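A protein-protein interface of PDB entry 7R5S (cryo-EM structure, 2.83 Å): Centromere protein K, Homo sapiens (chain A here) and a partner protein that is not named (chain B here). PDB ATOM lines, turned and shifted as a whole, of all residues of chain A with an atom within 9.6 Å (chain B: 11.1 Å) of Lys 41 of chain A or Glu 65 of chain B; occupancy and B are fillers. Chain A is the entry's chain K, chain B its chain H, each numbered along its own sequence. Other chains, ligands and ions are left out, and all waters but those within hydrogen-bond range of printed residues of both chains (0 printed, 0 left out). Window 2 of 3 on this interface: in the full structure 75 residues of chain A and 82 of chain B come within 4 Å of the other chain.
The backbone carbonyl oxygen (O) of Tyr 57 of chain B is in hydrogen-bond range of the side-chain sulfur (SG) of Cys 38 of chain A (3.5 Å).
The side-chain amino group of Lys 58 of chain B is in salt-bridge range of the side-chain carboxylate of Asp 34 of chain A (3.7 Å).
OE2 of Glu 65 of chain B is in salt-bridge range of NZ of Lys 41 of chain A (2.9 Å).
Among the printed residues, pairs that only touch across the chains: Met 35 of chain A with Leu 54 of chain B (3.9 Å), Met 35 of chain A with Tyr 57 of chain B (3.6 Å), Cys 38 of chain A with Lys 58 of chain B (3.9 Å), Cys 38 of chain A with Val 61 of chain B (3.4 Å), Gln 39 of chain A with Tyr 57 of chain B (3.5 Å), Lys 41 of chain A with Val 61 of chain B (3.97 Å), Leu 42 of chain A with Met 60 of chain B (3.8 Å), Leu 42 of chain A with Val 61 of chain B (3.6 Å), Cys 66 of chain A with Met 60 of chain B (3.6 Å), Ala 69 of chain A with Ser 59 of chain B (3.7 Å), Ala 69 of chain A with Ala 63 of chain B (3.8 Å), Gln 73 of chain A with Lys 58 of chain B (3.9 Å), Gln 73 of chain A with Ser 59 of chain B (3.9 Å) and Gln 73 of chain A with Asp 62 of chain B (3.95 Å).
Of the 18 printed residues of chain A, 9 touch a printed residue of chain B.
Hydrophobic or aromatic side chains of chain A within 4 Å of the printed part of chain B: Met 35, Leu 42 and Ala 69.
Of the 10 printed residues of chain B, 9 touch a printed residue of chain A.
Among the printed residues, Asp or Glu carboxylates within 4 Å of a Lys or Arg side-chain nitrogen of the other chain: Asp 34 of chain A with Lys 58 of chain B and Lys 41 of chain A with Glu 65 of chain B.
O of Val 61 of chain B lies within hydrogen-bond range of OG of Ser 64 of chain B (3.0 Å).
Of chain A, only Lys 41 (2.9 Å) comes within 4 Å of Glu 65 of chain B.
Of chain B, only Tyr 57 (3.5 Å), Lys 58 (3.9 Å) and Val 61 (3.4 Å) come within 4 Å of Cys 38 of chain A.
No residue of chain B comes within 4 Å of Asn 40 of chain A.
No residue of chain B comes within 4 Å of Ser 43 of chain A.
No residue of chain A comes within 4 Å of Ser 64 of chain B.
Printed residues of chain B within 4 Å of Gln 39 of chain A: Tyr 57.
Printed residues of chain A within 4 Å of Lys 58 of chain B: Asp 34 (3.7 Å), Cys 38 (3.9 Å) and Gln 73 (3.9 Å).
The nearest printed residue of chain A that does not touch Asp 62 of chain B is Ala 69 of chain A (4.3 Å).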
ATOM      1  N   LYS A  33       9.879 -19.098 -25.754  1.00  0.00           N
ATOM      2  CA  LYS A  33      10.209 -18.911 -27.163  1.00  0.00           C
ATOM      3  C   LYS A  33      11.624 -19.393 -27.465  1.00  0.00           C
ATOM      4  O   LYS A  33      11.867 -20.043 -28.493  1.00  0.00           O
ATOM      5  CB  LYS A  33      10.046 -17.440 -27.549  1.00  0.00           C
ATOM      6  CG  LYS A  33      10.133 -17.168 -29.044  1.00  0.00           C
ATOM      7  CD  LYS A  33      11.494 -16.612 -29.435  1.00  0.00           C
ATOM      8  CE  LYS A  33      11.771 -15.286 -28.746  1.00  0.00           C
ATOM      9  NZ  LYS A  33      13.090 -14.719 -29.144  1.00  0.00           N
ATOM     10  N   ASP A  34      12.573 -19.083 -26.576  1.00  0.00           N
ATOM     11  CA  ASP A  34      13.944 -19.544 -26.764  1.00  0.00           C
ATOM     12  C   ASP A  34      14.014 -21.066 -26.730  1.00  0.00           C
ATOM     13  O   ASP A  34      14.738 -21.679 -27.523  1.00  0.00           O
ATOM     14  CB  ASP A  34      14.848 -18.933 -25.689  1.00  0.00           C
ATOM     15  CG  ASP A  34      16.323 -18.989 -26.055  1.00  0.00           C
ATOM     16  OD1 ASP A  34      16.742 -19.934 -26.754  1.00  0.00           O
ATOM     17  OD2 ASP A  34      17.069 -18.080 -25.636  1.00  0.00           O
ATOM     18  N   MET A  35      13.249 -21.695 -25.834  1.00  0.00           N
ATOM     19  CA  MET A  35      13.245 -23.153 -25.757  1.00  0.00           C
ATOM     20  C   MET A  35      12.609 -23.772 -26.996  1.00  0.00           C
ATOM     21  O   MET A  35      13.059 -24.819 -27.474  1.00  0.00           O
ATOM     22  CB  MET A  35      12.520 -23.606 -24.491  1.00  0.00           C
ATOM     23  CG  MET A  35      12.545 -25.106 -24.258  1.00  0.00           C
ATOM     24  SD  MET A  35      12.162 -25.545 -22.552  1.00  0.00           S
ATOM     25  CE  MET A  35      10.627 -24.658 -22.311  1.00  0.00           C
ATOM     26  N   GLU A  36      11.563 -23.138 -27.532  1.00  0.00           N
ATOM     27  CA  GLU A  36      10.956 -23.626 -28.767  1.00  0.00           C
ATOM     28  C   GLU A  36      11.938 -23.554 -29.927  1.00  0.00           C
ATOM     29  O   GLU A  36      12.057 -24.504 -30.711  1.00  0.00           O
ATOM     30  CB  GLU A  36       9.693 -22.826 -29.087  1.00  0.00           C
ATOM     31  CG  GLU A  36       8.509 -23.144 -28.192  1.00  0.00           C
ATOM     32  CD  GLU A  36       7.276 -22.341 -28.555  1.00  0.00           C
ATOM     33  OE1 GLU A  36       7.372 -21.471 -29.445  1.00  0.00           O
ATOM     34  OE2 GLU A  36       6.210 -22.582 -27.951  1.00  0.00           O
ATOM     35  N   GLU A  37      12.651 -22.432 -30.055  1.00  0.00           N
ATOM     36  CA  GLU A  37      13.659 -22.321 -31.106  1.00  0.00           C
ATOM     37  C   GLU A  37      14.774 -23.342 -30.910  1.00  0.00           C
ATOM     38  O   GLU A  37      15.261 -23.938 -31.879  1.00  0.00           O
ATOM     39  CB  GLU A  37      14.228 -20.903 -31.143  1.00  0.00           C
ATOM     40  CG  GLU A  37      13.233 -19.848 -31.596  1.00  0.00           C
ATOM     41  CD  GLU A  37      13.859 -18.474 -31.725  1.00  0.00           C
ATOM     42  OE1 GLU A  37      15.029 -18.314 -31.318  1.00  0.00           O
ATOM     43  OE2 GLU A  37      13.183 -17.555 -32.233  1.00  0.00           O
ATOM     44  N   CYS A  38      15.179 -23.567 -29.658  1.00  0.00           N
ATOM     45  CA  CYS A  38      16.220 -24.544 -29.364  1.00  0.00           C
ATOM     46  C   CYS A  38      15.784 -25.949 -29.766  1.00  0.00           C
ATOM     47  O   CYS A  38      16.566 -26.706 -30.354  1.00  0.00           O
ATOM     48  CB  CYS A  38      16.564 -24.488 -27.877  1.00  0.00           C
ATOM     49  SG  CYS A  38      18.253 -24.946 -27.451  1.00  0.00           S
ATOM     50  N   GLN A  39      14.535 -26.309 -29.466  1.00  0.00           N
ATOM     51  CA  GLN A  39      14.028 -27.625 -29.843  1.00  0.00           C
ATOM     52  C   GLN A  39      13.909 -27.759 -31.356  1.00  0.00           C
ATOM     53  O   GLN A  39      14.221 -28.816 -31.917  1.00  0.00           O
ATOM     54  CB  GLN A  39      12.678 -27.879 -29.173  1.00  0.00           C
ATOM     55  CG  GLN A  39      12.066 -29.231 -29.502  1.00  0.00           C
ATOM     56  CD  GLN A  39      10.744 -29.108 -30.231  1.00  0.00           C
ATOM     57  OE1 GLN A  39      10.187 -28.018 -30.351  1.00  0.00           O
ATOM     58  NE2 GLN A  39      10.234 -30.230 -30.724  1.00  0.00           N
ATOM     59  N   ASN A  40      13.454 -26.701 -32.034  1.00  0.00           N
ATOM     60  CA  ASN A  40      13.362 -26.746 -33.490  1.00  0.00           C
ATOM     61  C   ASN A  40      14.737 -26.908 -34.123  1.00  0.00           C
ATOM     62  O   ASN A  40      14.879 -27.571 -35.157  1.00  0.00           O
ATOM     63  CB  ASN A  40      12.674 -25.486 -34.014  1.00  0.00           C
ATOM     64  CG  ASN A  40      11.172 -25.517 -33.817  1.00  0.00           C
ATOM     65  OD1 ASN A  40      10.433 -26.000 -34.675  1.00  0.00           O
ATOM     66  ND2 ASN A  40      10.713 -25.002 -32.683  1.00  0.00           N
ATOM     67  N   LYS A  41      15.764 -26.308 -33.518  1.00  0.00           N
ATOM     68  CA  LYS A  41      17.117 -26.467 -34.043  1.00  0.00           C
ATOM     69  C   LYS A  41      17.661 -27.862 -33.758  1.00  0.00           C
ATOM     70  O   LYS A  41      18.346 -28.451 -34.601  1.00  0.00           O
ATOM     71  CB  LYS A  41      18.037 -25.397 -33.457  1.00  0.00           C
ATOM     72  CG  LYS A  41      19.480 -25.493 -33.928  1.00  0.00           C
ATOM     73  CD  LYS A  41      20.350 -24.437 -33.267  1.00  0.00           C
ATOM     74  CE  LYS A  41      21.799 -24.568 -33.704  1.00  0.00           C
ATOM     75  NZ  LYS A  41      22.674 -23.557 -33.049  1.00  0.00           N
ATOM     76  N   LEU A  42      17.363 -28.407 -32.576  1.00  0.00           N
ATOM     77  CA  LEU A  42      17.876 -29.724 -32.211  1.00  0.00           C
ATOM     78  C   LEU A  42      17.165 -30.853 -32.947  1.00  0.00           C
ATOM     79  O   LEU A  42      17.741 -31.937 -33.097  1.00  0.00           O
ATOM     80  CB  LEU A  42      17.758 -29.928 -30.698  1.00  0.00           C
ATOM     81  CG  LEU A  42      18.429 -31.155 -30.074  1.00  0.00           C
ATOM     82  CD1 LEU A  42      19.102 -30.787 -28.764  1.00  0.00           C
ATOM     83  CD2 LEU A  42      17.420 -32.270 -29.853  1.00  0.00           C
ATOM     84  N   SER A  43      15.940 -30.629 -33.418  1.00  0.00           N
ATOM     85  CA  SER A  43      15.187 -31.696 -34.080  1.00  0.00           C
ATOM     86  C   SER A  43      15.712 -32.045 -35.477  1.00  0.00           C
ATOM     87  O   SER A  43      15.038 -32.817 -36.172  1.00  0.00           O
ATOM     88  CB  SER A  43      13.709 -31.311 -34.166  1.00  0.00           C
ATOM     89  OG  SER A  43      13.053 -32.040 -35.188  1.00  0.00           O
ATOM     90  N   LEU A  44      16.855 -31.531 -35.924  1.00  0.00           N
ATOM     91  CA  LEU A  44      17.392 -31.838 -37.242  1.00  0.00           C
ATOM     92  C   LEU A  44      18.555 -32.822 -37.192  1.00  0.00           C
ATOM     93  O   LEU A  44      19.247 -32.998 -38.200  1.00  0.00           O
ATOM     94  CB  LEU A  44      17.829 -30.552 -37.949  1.00  0.00           C
ATOM     95  CG  LEU A  44      16.790 -29.831 -38.813  1.00  0.00           C
ATOM     96  CD1 LEU A  44      15.627 -29.317 -37.977  1.00  0.00           C
ATOM     97  CD2 LEU A  44      17.440 -28.696 -39.588  1.00  0.00           C
ATOM     98  N   ILE A  45      18.787 -33.461 -36.049  1.00  0.00           N
ATOM     99  CA  ILE A  45      19.885 -34.408 -35.881  1.00  0.00           C
ATOM    100  C   ILE A  45      19.340 -35.823 -36.007  1.00  0.00           C
ATOM    101  O   ILE A  45      18.261 -36.135 -35.488  1.00  0.00           O
ATOM    102  CB  ILE A  45      20.590 -34.203 -34.526  1.00  0.00           C
ATOM    103  CG1 ILE A  45      20.971 -32.733 -34.340  1.00  0.00           C
ATOM    104  CG2 ILE A  45      21.825 -35.084 -34.425  1.00  0.00           C
ATOM    105  CD1 ILE A  45      21.909 -32.208 -35.403  1.00  0.00           C
ATOM    106  N   GLY A  46      20.089 -36.684 -36.700  1.00  0.00           N
ATOM    107  CA  GLY A  46      19.668 -38.057 -36.869  1.00  0.00           C
ATOM    108  C   GLY A  46      19.907 -38.903 -35.631  1.00  0.00           C
ATOM    109  O   GLY A  46      20.691 -38.562 -34.746  1.00  0.00           O
ATOM    110  N   LYS A  65      31.823 -34.737 -24.208  1.00  0.00           N
ATOM    111  CA  LYS A  65      31.288 -33.608 -24.966  1.00  0.00           C
ATOM    112  C   LYS A  65      30.226 -32.859 -24.166  1.00  0.00           C
ATOM    113  O   LYS A  65      30.218 -31.621 -24.120  1.00  0.00           O
ATOM    114  CB  LYS A  65      30.716 -34.095 -26.297  1.00  0.00           C
ATOM    115  CG  LYS A  65      31.754 -34.665 -27.246  1.00  0.00           C
ATOM    116  CD  LYS A  65      31.121 -35.098 -28.557  1.00  0.00           C
ATOM    117  CE  LYS A  65      32.161 -35.645 -29.519  1.00  0.00           C
ATOM    118  NZ  LYS A  65      31.548 -36.115 -30.791  1.00  0.00           N
ATOM    119  N   CYS A  66      29.322 -33.598 -23.518  1.00  0.00           N
ATOM    120  CA  CYS A  66      28.251 -32.964 -22.761  1.00  0.00           C
ATOM    121  C   CYS A  66      28.786 -32.201 -21.556  1.00  0.00           C
ATOM    122  O   CYS A  66      28.292 -31.110 -21.250  1.00  0.00           O
ATOM    123  CB  CYS A  66      27.231 -34.013 -22.318  1.00  0.00           C
ATOM    124  SG  CYS A  66      26.091 -34.524 -23.622  1.00  0.00           S
ATOM    125  N   ALA A  69      30.321 -28.989 -22.773  1.00  0.00           N
ATOM    126  CA  ALA A  69      29.298 -27.997 -23.092  1.00  0.00           C
ATOM    127  C   ALA A  69      28.695 -27.396 -21.825  1.00  0.00           C
ATOM    128  O   ALA A  69      28.515 -26.174 -21.727  1.00  0.00           O
ATOM    129  CB  ALA A  69      28.209 -28.627 -23.961  1.00  0.00           C
ATOM    130  N   GLN A  73      28.281 -23.560 -20.361  1.00  0.00           N
ATOM    131  CA  GLN A  73      26.926 -23.083 -20.102  1.00  0.00           C
ATOM    132  C   GLN A  73      26.772 -22.568 -18.676  1.00  0.00           C
ATOM    133  O   GLN A  73      26.040 -21.599 -18.443  1.00  0.00           O
ATOM    134  CB  GLN A  73      25.914 -24.194 -20.379  1.00  0.00           C
ATOM    135  CG  GLN A  73      25.623 -24.404 -21.854  1.00  0.00           C
ATOM    136  CD  GLN A  73      25.047 -23.167 -22.515  1.00  0.00           C
ATOM    137  OE1 GLN A  73      24.288 -22.418 -21.900  1.00  0.00           O
ATOM    138  NE2 GLN A  73      25.411 -22.945 -23.772  1.00  0.00           N
ATOM    139  N   LEU B  54      15.660 -24.865 -19.833  1.00  0.00           N
ATOM    140  CA  LEU B  54      16.339 -24.151 -20.906  1.00  0.00           C
ATOM    141  C   LEU B  54      17.848 -24.330 -20.841  1.00  0.00           C
ATOM    142  O   LEU B  54      18.501 -24.398 -21.888  1.00  0.00           O
ATOM    143  CB  LEU B  54      15.983 -22.665 -20.852  1.00  0.00           C
ATOM    144  CG  LEU B  54      16.566 -21.774 -21.950  1.00  0.00           C
ATOM    145  CD1 LEU B  54      16.153 -22.276 -23.323  1.00  0.00           C
ATOM    146  CD2 LEU B  54      16.135 -20.330 -21.752  1.00  0.00           C
ATOM    147  N   TYR B  57      18.460 -27.659 -22.437  1.00  0.00           N
ATOM    148  CA  TYR B  57      18.248 -27.570 -23.880  1.00  0.00           C
ATOM    149  C   TYR B  57      19.438 -26.910 -24.570  1.00  0.00           C
ATOM    150  O   TYR B  57      19.939 -27.406 -25.590  1.00  0.00           O
ATOM    151  CB  TYR B  57      16.962 -26.799 -24.175  1.00  0.00           C
ATOM    152  CG  TYR B  57      15.836 -27.659 -24.698  1.00  0.00           C
ATOM    153  CD1 TYR B  57      15.871 -28.174 -25.986  1.00  0.00           C
ATOM    154  CD2 TYR B  57      14.732 -27.949 -23.907  1.00  0.00           C
ATOM    155  CE1 TYR B  57      14.844 -28.960 -26.469  1.00  0.00           C
ATOM    156  CE2 TYR B  57      13.700 -28.733 -24.383  1.00  0.00           C
ATOM    157  CZ  TYR B  57      13.760 -29.234 -25.664  1.00  0.00           C
ATOM    158  OH  TYR B  57      12.735 -30.016 -26.142  1.00  0.00           O
ATOM    159  N   LYS B  58      19.904 -25.784 -24.024  1.00  0.00           N
ATOM    160  CA  LYS B  58      21.034 -25.081 -24.620  1.00  0.00           C
ATOM    161  C   LYS B  58      22.304 -25.919 -24.555  1.00  0.00           C
ATOM    162  O   LYS B  58      23.096 -25.931 -25.503  1.00  0.00           O
ATOM    163  CB  LYS B  58      21.242 -23.735 -23.929  1.00  0.00           C
ATOM    164  CG  LYS B  58      20.291 -22.647 -24.392  1.00  0.00           C
ATOM    165  CD  LYS B  58      20.722 -21.285 -23.877  1.00  0.00           C
ATOM    166  CE  LYS B  58      19.876 -20.176 -24.480  1.00  0.00           C
ATOM    167  NZ  LYS B  58      20.323 -18.831 -24.023  1.00  0.00           N
ATOM    168  N   SER B  59      22.511 -26.636 -23.446  1.00  0.00           N
ATOM    169  CA  SER B  59      23.688 -27.491 -23.338  1.00  0.00           C
ATOM    170  C   SER B  59      23.649 -28.614 -24.366  1.00  0.00           C
ATOM    171  O   SER B  59      24.671 -28.934 -24.985  1.00  0.00           O
ATOM    172  CB  SER B  59      23.796 -28.061 -21.924  1.00  0.00           C
ATOM    173  OG  SER B  59      24.600 -29.227 -21.906  1.00  0.00           O
ATOM    174  N   MET B  60      22.476 -29.217 -24.572  1.00  0.00           N
ATOM    175  CA  MET B  60      22.357 -30.277 -25.569  1.00  0.00           C
ATOM    176  C   MET B  60      22.610 -29.746 -26.974  1.00  0.00           C
ATOM    177  O   MET B  60      23.302 -30.392 -27.772  1.00  0.00           O
ATOM    178  CB  MET B  60      20.977 -30.930 -25.486  1.00  0.00           C
ATOM    179  CG  MET B  60      20.763 -31.789 -24.249  1.00  0.00           C
ATOM    180  SD  MET B  60      21.821 -33.248 -24.210  1.00  0.00           S
ATOM    181  CE  MET B  60      23.004 -32.774 -22.952  1.00  0.00           C
ATOM    182  N   VAL B  61      22.067 -28.570 -27.295  1.00  0.00           N
ATOM    183  CA  VAL B  61      22.278 -28.005 -28.627  1.00  0.00           C
ATOM    184  C   VAL B  61      23.746 -27.643 -28.832  1.00  0.00           C
ATOM    185  O   VAL B  61      24.301 -27.833 -29.921  1.00  0.00           O
ATOM    186  CB  VAL B  61      21.348 -26.799 -28.854  1.00  0.00           C
ATOM    187  CG1 VAL B  61      21.913 -25.871 -29.915  1.00  0.00           C
ATOM    188  CG2 VAL B  61      19.977 -27.287 -29.281  1.00  0.00           C
ATOM    189  N   ASP B  62      24.406 -27.142 -27.785  1.00  0.00           N
ATOM    190  CA  ASP B  62      25.817 -26.795 -27.910  1.00  0.00           C
ATOM    191  C   ASP B  62      26.682 -28.041 -28.060  1.00  0.00           C
ATOM    192  O   ASP B  62      27.668 -28.032 -28.806  1.00  0.00           O
ATOM    193  CB  ASP B  62      26.264 -25.972 -26.702  1.00  0.00           C
ATOM    194  CG  ASP B  62      27.598 -25.290 -26.923  1.00  0.00           C
ATOM    195  OD1 ASP B  62      28.081 -25.279 -28.076  1.00  0.00           O
ATOM    196  OD2 ASP B  62      28.166 -24.762 -25.944  1.00  0.00           O
ATOM    197  N   ALA B  63      26.329 -29.123 -27.363  1.00  0.00           N
ATOM    198  CA  ALA B  63      27.087 -30.363 -27.470  1.00  0.00           C
ATOM    199  C   ALA B  63      26.816 -31.110 -28.769  1.00  0.00           C
ATOM    200  O   ALA B  63      27.654 -31.915 -29.189  1.00  0.00           O
ATOM    201  CB  ALA B  63      26.779 -31.275 -26.282  1.00  0.00           C
ATOM    202  N   SER B  64      25.670 -30.866 -29.410  1.00  0.00           N
ATOM    203  CA  SER B  64      25.372 -31.545 -30.668  1.00  0.00           C
ATOM    204  C   SER B  64      26.326 -31.109 -31.774  1.00  0.00           C
ATOM    205  O   SER B  64      26.717 -31.922 -32.620  1.00  0.00           O
ATOM    206  CB  SER B  64      23.923 -31.284 -31.077  1.00  0.00           C
ATOM    207  OG  SER B  64      23.815 -30.091 -31.834  1.00  0.00           O
ATOM    208  N   GLU B  65      26.709 -29.836 -31.785  1.00  0.00           N
ATOM    209  CA  GLU B  65      27.621 -29.318 -32.799  1.00  0.00           C
ATOM    210  C   GLU B  65      29.039 -29.833 -32.581  1.00  0.00           C
ATOM    211  O   GLU B  65      29.983 -29.052 -32.469  1.00  0.00           O
ATOM    212  CB  GLU B  65      27.612 -27.788 -32.795  1.00  0.00           C
ATOM    213  CG  GLU B  65      26.241 -27.177 -33.023  1.00  0.00           C
ATOM    214  CD  GLU B  65      26.243 -25.670 -32.862  1.00  0.00           C
ATOM    215  OE1 GLU B  65      27.313 -25.106 -32.552  1.00  0.00           O
ATOM    216  OE2 GLU B  65      25.175 -25.049 -33.044  1.00  0.00           O
